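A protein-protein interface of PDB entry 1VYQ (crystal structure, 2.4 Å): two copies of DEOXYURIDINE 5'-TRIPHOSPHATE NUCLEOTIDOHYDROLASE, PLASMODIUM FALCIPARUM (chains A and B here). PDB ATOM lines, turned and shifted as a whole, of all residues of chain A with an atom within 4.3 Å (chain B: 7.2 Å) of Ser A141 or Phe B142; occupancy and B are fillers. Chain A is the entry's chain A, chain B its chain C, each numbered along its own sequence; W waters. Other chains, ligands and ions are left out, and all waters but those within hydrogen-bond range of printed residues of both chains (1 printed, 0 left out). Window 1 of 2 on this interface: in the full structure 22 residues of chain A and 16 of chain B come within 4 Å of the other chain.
The backbone carbonyl oxygen (O) of Phe A142 lies close to the backbone carbonyl oxygen (O) of Phe B142, 3.5 Å away.
OG of Ser A141 sits close to SD of Met A1. The side-chain hydroxyl (OG) of Ser A141 sits at hydrogen-bond distance from the side-chain amide oxygen (OE1) of Gln A57. The side-chain hydroxyl (OG) of Ser A141 lies within hydrogen-bond range of the side-chain hydroxyl (OG1) of Thr A143, at 3.2 Å. The side-chain hydroxyl (OG1) of Thr A143 lies close to the backbone NH (N) of Glu A145 (3.0 Å).
Ser A141 touches Phe B142 (O to CE1, 3.5 Å). Thr A143 touches Phe B142 (O to CB, 3.5 Å). Phe B142 touches Gly A144 (CD1 to N, 3.3 Å).
Of the printed residues of chain B, Ser A141 touches Phe B142 (3.5 Å). Printed residues of chain B within 4 Å of Phe A142: Phe B142. Printed residues of chain B within 4 Å of Thr A143: Phe B142 (3.5 Å). Of the printed residues of chain B, Gly A144 touches Phe B142 (3.3 Å). Leu A147 touches none of the printed residues of chain B. Of the printed residues of chain A, Phe B142 touches Ser A141, Phe A142, Thr A143 and Gly A144. The nearest printed residue of chain A that does not touch Phe B142 is Val A140 (4.01 Å).
Hydrophobic or aromatic side chains of chain B that line the printed part of chain A: Phe B142. Printed residues of chain A that touch a printed residue of chain B: Ser A141, Phe A142, Thr A143 and Gly A144. Among the printed residues, 4 pairs touch across the chains.
Ser A141 touches Phe B142, but with the chains exchanged Phe A142 does not touch Ser B141 (6.8 Å). Phe B142 touches its own counterpart, Phe A142. Thr A143 touches Phe B142, but with the chains exchanged Phe A142 does not touch Thr B143 (5.3 Å). Gly A144 touches Phe B142, but with the chains exchanged Phe A142 does not touch Gly B144 (7.4 Å). Of the 4 pairs that touch across the chains among the printed residues, 1 has its exchanged pair printed and touching as well.
Water W1 lies within hydrogen-bond range of the backbone carbonyl oxygen (O) of Phe A142 and the backbone carbonyl oxygen (O) of Phe B142.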
ATOM      1  N   MET A   1      29.978  -4.217  11.720  1.00  0.00           N
ATOM      2  CA  MET A   1      29.894  -3.000  12.577  1.00  0.00           C
ATOM      3  C   MET A   1      31.283  -2.385  12.711  1.00  0.00           C
ATOM      4  O   MET A   1      32.310  -3.087  12.668  1.00  0.00           O
ATOM      5  CB  MET A   1      29.287  -3.364  13.957  1.00  0.00           C
ATOM      6  CG  MET A   1      29.312  -2.277  15.060  1.00  0.00           C
ATOM      7  SD  MET A   1      28.646  -2.892  16.692  1.00  0.00           S
ATOM      8  CE  MET A   1      30.176  -3.097  17.654  1.00  0.00           C
ATOM      9  N   GLN A  57      26.635   1.308  12.308  1.00  0.00           N
ATOM     10  CA  GLN A  57      25.963   0.283  11.500  1.00  0.00           C
ATOM     11  C   GLN A  57      25.097   0.949  10.464  1.00  0.00           C
ATOM     12  O   GLN A  57      24.530   2.004  10.729  1.00  0.00           O
ATOM     13  CB  GLN A  57      25.028  -0.573  12.378  1.00  0.00           C
ATOM     14  CG  GLN A  57      25.723  -1.749  13.069  1.00  0.00           C
ATOM     15  CD  GLN A  57      24.869  -2.438  14.146  1.00  0.00           C
ATOM     16  OE1 GLN A  57      25.233  -3.533  14.648  1.00  0.00           O
ATOM     17  NE2 GLN A  57      23.735  -1.815  14.505  1.00  0.00           N
ATOM     18  N   VAL A 140      31.089  -6.497  21.290  1.00  0.00           N
ATOM     19  CA  VAL A 140      30.367  -7.190  20.271  1.00  0.00           C
ATOM     20  C   VAL A 140      29.088  -6.472  19.857  1.00  0.00           C
ATOM     21  O   VAL A 140      28.475  -5.730  20.625  1.00  0.00           O
ATOM     22  CB  VAL A 140      30.192  -8.738  20.578  1.00  0.00           C
ATOM     23  CG1 VAL A 140      30.978  -9.164  21.783  1.00  0.00           C
ATOM     24  CG2 VAL A 140      28.802  -9.154  20.716  1.00  0.00           C
ATOM     25  N   SER A 141      28.779  -6.636  18.576  1.00  0.00           N
ATOM     26  CA  SER A 141      27.583  -6.107  17.958  1.00  0.00           C
ATOM     27  C   SER A 141      26.445  -7.024  18.285  1.00  0.00           C
ATOM     28  O   SER A 141      26.630  -8.241  18.335  1.00  0.00           O
ATOM     29  CB  SER A 141      27.761  -6.141  16.449  1.00  0.00           C
ATOM     30  OG  SER A 141      26.663  -5.610  15.756  1.00  0.00           O
ATOM     31  N   PHE A 142      25.274  -6.444  18.489  1.00  0.00           N
ATOM     32  CA  PHE A 142      24.005  -7.184  18.497  1.00  0.00           C
ATOM     33  C   PHE A 142      23.849  -8.133  17.327  1.00  0.00           C
ATOM     34  O   PHE A 142      23.265  -9.191  17.488  1.00  0.00           O
ATOM     35  CB  PHE A 142      22.789  -6.208  18.499  1.00  0.00           C
ATOM     36  CG  PHE A 142      22.353  -5.795  19.880  1.00  0.00           C
ATOM     37  CD1 PHE A 142      21.567  -6.646  20.645  1.00  0.00           C
ATOM     38  CD2 PHE A 142      22.751  -4.569  20.413  1.00  0.00           C
ATOM     39  CE1 PHE A 142      21.187  -6.285  21.891  1.00  0.00           C
ATOM     40  CE2 PHE A 142      22.391  -4.202  21.653  1.00  0.00           C
ATOM     41  CZ  PHE A 142      21.602  -5.030  22.411  1.00  0.00           C
ATOM     42  N   THR A 143      24.282  -7.771  16.130  1.00  0.00           N
ATOM     43  CA  THR A 143      24.152  -8.758  15.018  1.00  0.00           C
ATOM     44  C   THR A 143      25.123  -9.958  15.103  1.00  0.00           C
ATOM     45  O   THR A 143      24.998 -10.896  14.360  1.00  0.00           O
ATOM     46  CB  THR A 143      24.412  -8.088  13.657  1.00  0.00           C
ATOM     47  OG1 THR A 143      25.814  -7.759  13.545  1.00  0.00           O
ATOM     48  CG2 THR A 143      23.751  -6.741  13.542  1.00  0.00           C
ATOM     49  N   GLY A 144      26.147  -9.899  15.931  1.00  0.00           N
ATOM     50  CA  GLY A 144      27.189 -10.909  15.915  1.00  0.00           C
ATOM     51  C   GLY A 144      28.053 -10.884  14.664  1.00  0.00           C
ATOM     52  O   GLY A 144      28.806 -11.803  14.434  1.00  0.00           O
ATOM     53  N   GLU A 145      27.965  -9.815  13.878  1.00  0.00           N
ATOM     54  CA  GLU A 145      28.753  -9.672  12.669  1.00  0.00           C
ATOM     55  C   GLU A 145      30.244  -9.347  13.006  1.00  0.00           C
ATOM     56  O   GLU A 145      30.568  -8.982  14.136  1.00  0.00           O
ATOM     57  CB  GLU A 145      28.116  -8.602  11.732  1.00  0.00           C
ATOM     58  CG  GLU A 145      28.406  -7.109  12.114  1.00  0.00           C
ATOM     59  CD  GLU A 145      27.295  -6.099  11.784  1.00  0.00           C
ATOM     60  OE1 GLU A 145      27.564  -4.890  11.690  1.00  0.00           O
ATOM     61  OE2 GLU A 145      26.127  -6.483  11.652  1.00  0.00           O
ATOM     62  N   LEU A 147      33.595  -7.243  13.216  1.00  0.00           N
ATOM     63  CA  LEU A 147      33.810  -5.912  13.737  1.00  0.00           C
ATOM     64  C   LEU A 147      35.036  -5.285  13.095  1.00  0.00           C
ATOM     65  O   LEU A 147      36.044  -5.956  12.922  1.00  0.00           O
ATOM     66  CB  LEU A 147      34.113  -5.989  15.241  1.00  0.00           C
ATOM     67  CG  LEU A 147      33.010  -6.217  16.266  1.00  0.00           C
ATOM     68  CD1 LEU A 147      33.174  -5.233  17.365  1.00  0.00           C
ATOM     69  CD2 LEU A 147      31.645  -6.090  15.660  1.00  0.00           C
ATOM     70  N   MET B   1      18.610 -19.708  11.890  1.00  0.00           N
ATOM     71  CA  MET B   1      19.972 -20.320  11.894  1.00  0.00           C
ATOM     72  C   MET B   1      19.845 -21.826  11.741  1.00  0.00           C
ATOM     73  O   MET B   1      18.883 -22.431  12.242  1.00  0.00           O
ATOM     74  CB  MET B   1      20.715 -19.960  13.194  1.00  0.00           C
ATOM     75  CG  MET B   1      22.135 -20.472  13.340  1.00  0.00           C
ATOM     76  SD  MET B   1      23.059 -19.539  14.626  1.00  0.00           S
ATOM     77  CE  MET B   1      22.481 -20.436  16.207  1.00  0.00           C
ATOM     78  N   GLN B  57      23.826 -19.121   8.328  1.00  0.00           N
ATOM     79  CA  GLN B  57      22.887 -18.003   8.381  1.00  0.00           C
ATOM     80  C   GLN B  57      22.989 -17.334   7.022  1.00  0.00           C
ATOM     81  O   GLN B  57      24.025 -17.382   6.385  1.00  0.00           O
ATOM     82  CB  GLN B  57      23.260 -16.973   9.481  1.00  0.00           C
ATOM     83  CG  GLN B  57      22.307 -16.892  10.739  1.00  0.00           C
ATOM     84  CD  GLN B  57      22.789 -15.851  11.808  1.00  0.00           C
ATOM     85  OE1 GLN B  57      22.483 -15.956  13.017  1.00  0.00           O
ATOM     86  NE2 GLN B  57      23.573 -14.858  11.346  1.00  0.00           N
ATOM     87  N   THR B  84      28.565 -18.403  10.928  1.00  0.00           N
ATOM     88  CA  THR B  84      28.406 -17.346  11.908  1.00  0.00           C
ATOM     89  C   THR B  84      28.754 -17.790  13.330  1.00  0.00           C
ATOM     90  O   THR B  84      28.874 -18.972  13.654  1.00  0.00           O
ATOM     91  CB  THR B  84      26.969 -16.715  11.798  1.00  0.00           C
ATOM     92  OG1 THR B  84      26.678 -15.868  12.914  1.00  0.00           O
ATOM     93  CG2 THR B  84      25.869 -17.756  11.926  1.00  0.00           C
ATOM     94  N   SER B  85      28.972 -16.784  14.155  1.00  0.00           N
ATOM     95  CA  SER B  85      29.078 -16.913  15.573  1.00  0.00           C
ATOM     96  C   SER B  85      27.709 -17.115  16.150  1.00  0.00           C
ATOM     97  O   SER B  85      26.697 -16.754  15.542  1.00  0.00           O
ATOM     98  CB  SER B  85      29.688 -15.657  16.131  1.00  0.00           C
ATOM     99  OG  SER B  85      30.941 -15.418  15.512  1.00  0.00           O
ATOM    100  N   PHE B  86      27.679 -17.745  17.317  1.00  0.00           N
ATOM    101  CA  PHE B  86      26.431 -17.994  17.990  1.00  0.00           C
ATOM    102  C   PHE B  86      26.685 -17.995  19.446  1.00  0.00           C
ATOM    103  O   PHE B  86      27.809 -17.888  19.843  1.00  0.00           O
ATOM    104  CB  PHE B  86      25.759 -19.314  17.525  1.00  0.00           C
ATOM    105  CG  PHE B  86      26.632 -20.546  17.659  1.00  0.00           C
ATOM    106  CD1 PHE B  86      27.608 -20.822  16.728  1.00  0.00           C
ATOM    107  CD2 PHE B  86      26.474 -21.413  18.729  1.00  0.00           C
ATOM    108  CE1 PHE B  86      28.399 -21.979  16.848  1.00  0.00           C
ATOM    109  CE2 PHE B  86      27.276 -22.566  18.876  1.00  0.00           C
ATOM    110  CZ  PHE B  86      28.238 -22.851  17.939  1.00  0.00           C
ATOM    111  N   LEU B  87      25.619 -18.138  20.228  1.00  0.00           N
ATOM    112  CA  LEU B  87      25.653 -17.911  21.646  1.00  0.00           C
ATOM    113  C   LEU B  87      25.261 -19.153  22.370  1.00  0.00           C
ATOM    114  O   LEU B  87      24.621 -20.045  21.833  1.00  0.00           O
ATOM    115  CB  LEU B  87      24.696 -16.796  22.032  1.00  0.00           C
ATOM    116  CG  LEU B  87      24.957 -15.488  21.311  1.00  0.00           C
ATOM    117  CD1 LEU B  87      23.688 -14.644  21.170  1.00  0.00           C
ATOM    118  CD2 LEU B  87      26.051 -14.710  22.051  1.00  0.00           C
ATOM    119  N   PHE B  89      23.501 -19.885  25.934  1.00  0.00           N
ATOM    120  CA  PHE B  89      22.770 -19.360  27.071  1.00  0.00           C
ATOM    121  C   PHE B  89      22.588 -20.382  28.137  1.00  0.00           C
ATOM    122  O   PHE B  89      22.405 -21.529  27.854  1.00  0.00           O
ATOM    123  CB  PHE B  89      21.373 -18.940  26.632  1.00  0.00           C
ATOM    124  CG  PHE B  89      21.330 -17.599  25.998  1.00  0.00           C
ATOM    125  CD1 PHE B  89      22.085 -17.329  24.864  1.00  0.00           C
ATOM    126  CD2 PHE B  89      20.557 -16.587  26.549  1.00  0.00           C
ATOM    127  CE1 PHE B  89      22.018 -16.121  24.270  1.00  0.00           C
ATOM    128  CE2 PHE B  89      20.501 -15.368  25.947  1.00  0.00           C
ATOM    129  CZ  PHE B  89      21.249 -15.133  24.815  1.00  0.00           C
ATOM    130  N   GLY B 106      27.998 -17.772  26.607  1.00  0.00           N
ATOM    131  CA  GLY B 106      29.053 -18.235  25.735  1.00  0.00           C
ATOM    132  C   GLY B 106      28.968 -17.550  24.387  1.00  0.00           C
ATOM    133  O   GLY B 106      27.854 -17.452  23.835  1.00  0.00           O
ATOM    134  N   LEU B 107      30.115 -17.034  23.905  1.00  0.00           N
ATOM    135  CA  LEU B 107      30.243 -16.617  22.508  1.00  0.00           C
ATOM    136  C   LEU B 107      31.217 -17.530  21.752  1.00  0.00           C
ATOM    137  O   LEU B 107      32.415 -17.621  22.068  1.00  0.00           O
ATOM    138  CB  LEU B 107      30.701 -15.172  22.407  1.00  0.00           C
ATOM    139  CG  LEU B 107      30.477 -14.328  21.144  1.00  0.00           C
ATOM    140  CD1 LEU B 107      31.461 -13.254  21.145  1.00  0.00           C
ATOM    141  CD2 LEU B 107      30.565 -15.070  19.867  1.00  0.00           C
ATOM    142  N   ILE B 108      30.659 -18.224  20.779  1.00  0.00           N
ATOM    143  CA  ILE B 108      31.364 -19.199  19.980  1.00  0.00           C
ATOM    144  C   ILE B 108      31.526 -18.544  18.646  1.00  0.00           C
ATOM    145  O   ILE B 108      30.540 -18.334  17.929  1.00  0.00           O
ATOM    146  CB  ILE B 108      30.553 -20.568  19.872  1.00  0.00           C
ATOM    147  CG1 ILE B 108      30.672 -21.339  21.182  1.00  0.00           C
ATOM    148  CG2 ILE B 108      31.108 -21.445  18.785  1.00  0.00           C
ATOM    149  CD1 ILE B 108      29.514 -21.316  21.996  1.00  0.00           C
ATOM    150  N   VAL B 140      21.682 -20.294  20.949  1.00  0.00           N
ATOM    151  CA  VAL B 140      20.782 -19.314  20.359  1.00  0.00           C
ATOM    152  C   VAL B 140      21.517 -18.493  19.323  1.00  0.00           C
ATOM    153  O   VAL B 140      22.736 -18.433  19.278  1.00  0.00           O
ATOM    154  CB  VAL B 140      19.943 -18.451  21.417  1.00  0.00           C
ATOM    155  CG1 VAL B 140      20.129 -18.864  22.815  1.00  0.00           C
ATOM    156  CG2 VAL B 140      20.097 -16.964  21.240  1.00  0.00           C
ATOM    157  N   SER B 141      20.760 -17.933  18.423  1.00  0.00           N
ATOM    158  CA  SER B 141      21.340 -17.162  17.346  1.00  0.00           C
ATOM    159  C   SER B 141      21.283 -15.722  17.843  1.00  0.00           C
ATOM    160  O   SER B 141      20.443 -15.382  18.676  1.00  0.00           O
ATOM    161  CB  SER B 141      20.534 -17.359  16.076  1.00  0.00           C
ATOM    162  OG  SER B 141      20.730 -16.304  15.156  1.00  0.00           O
ATOM    163  N   PHE B 142      22.211 -14.915  17.353  1.00  0.00           N
ATOM    164  CA  PHE B 142      22.272 -13.484  17.603  1.00  0.00           C
ATOM    165  C   PHE B 142      21.027 -12.771  17.168  1.00  0.00           C
ATOM    166  O   PHE B 142      20.801 -11.626  17.633  1.00  0.00           O
ATOM    167  CB  PHE B 142      23.426 -12.883  16.814  1.00  0.00           C
ATOM    168  CG  PHE B 142      24.685 -12.803  17.570  1.00  0.00           C
ATOM    169  CD1 PHE B 142      24.916 -11.726  18.450  1.00  0.00           C
ATOM    170  CD2 PHE B 142      25.658 -13.766  17.412  1.00  0.00           C
ATOM    171  CE1 PHE B 142      26.052 -11.636  19.168  1.00  0.00           C
ATOM    172  CE2 PHE B 142      26.877 -13.655  18.121  1.00  0.00           C
ATOM    173  CZ  PHE B 142      27.040 -12.602  19.019  1.00  0.00           C
ATOM    174  N   THR B 143      20.271 -13.386  16.239  1.00  0.00           N
ATOM    175  CA  THR B 143      18.943 -12.886  15.790  1.00  0.00           C
ATOM    176  C   THR B 143      17.764 -13.272  16.651  1.00  0.00           C
ATOM    177  O   THR B 143      16.701 -12.658  16.545  1.00  0.00           O
ATOM    178  CB  THR B 143      18.591 -13.332  14.316  1.00  0.00           C
ATOM    179  OG1 THR B 143      18.594 -14.763  14.175  1.00  0.00           O
ATOM    180  CG2 THR B 143      19.637 -12.953  13.358  1.00  0.00           C
ATOM    181  N   GLY B 144      17.917 -14.301  17.469  1.00  0.00           N
ATOM    182  CA  GLY B 144      16.788 -14.928  18.149  1.00  0.00           C
ATOM    183  C   GLY B 144      15.841 -15.642  17.173  1.00  0.00           C
ATOM    184  O   GLY B 144      14.706 -15.893  17.461  1.00  0.00           O
ATOM    185  N   GLU B 145      16.317 -15.961  15.986  1.00  0.00           N
ATOM    186  CA  GLU B 145      15.465 -16.621  15.037  1.00  0.00           C
ATOM    187  C   GLU B 145      15.449 -18.095  15.360  1.00  0.00           C
ATOM    188  O   GLU B 145      16.320 -18.616  16.044  1.00  0.00           O
ATOM    189  CB  GLU B 145      16.043 -16.400  13.639  1.00  0.00           C
ATOM    190  N   LEU B 147      15.871 -22.131  15.272  1.00  0.00           N
ATOM    191  CA  LEU B 147      17.096 -22.899  15.013  1.00  0.00           C
ATOM    192  C   LEU B 147      16.694 -24.240  14.390  1.00  0.00           C
ATOM    193  O   LEU B 147      15.742 -24.884  14.820  1.00  0.00           O
ATOM    194  CB  LEU B 147      17.855 -23.172  16.319  1.00  0.00           C
ATOM    195  CG  LEU B 147      18.672 -22.111  17.114  1.00  0.00           C
ATOM    196  CD1 LEU B 147      20.141 -22.550  17.305  1.00  0.00           C
ATOM    197  CD2 LEU B 147      18.677 -20.756  16.491  1.00  0.00           C
HETATM  198  O   HOH W   1      21.018  -9.358  16.543  1.00  0.00           O
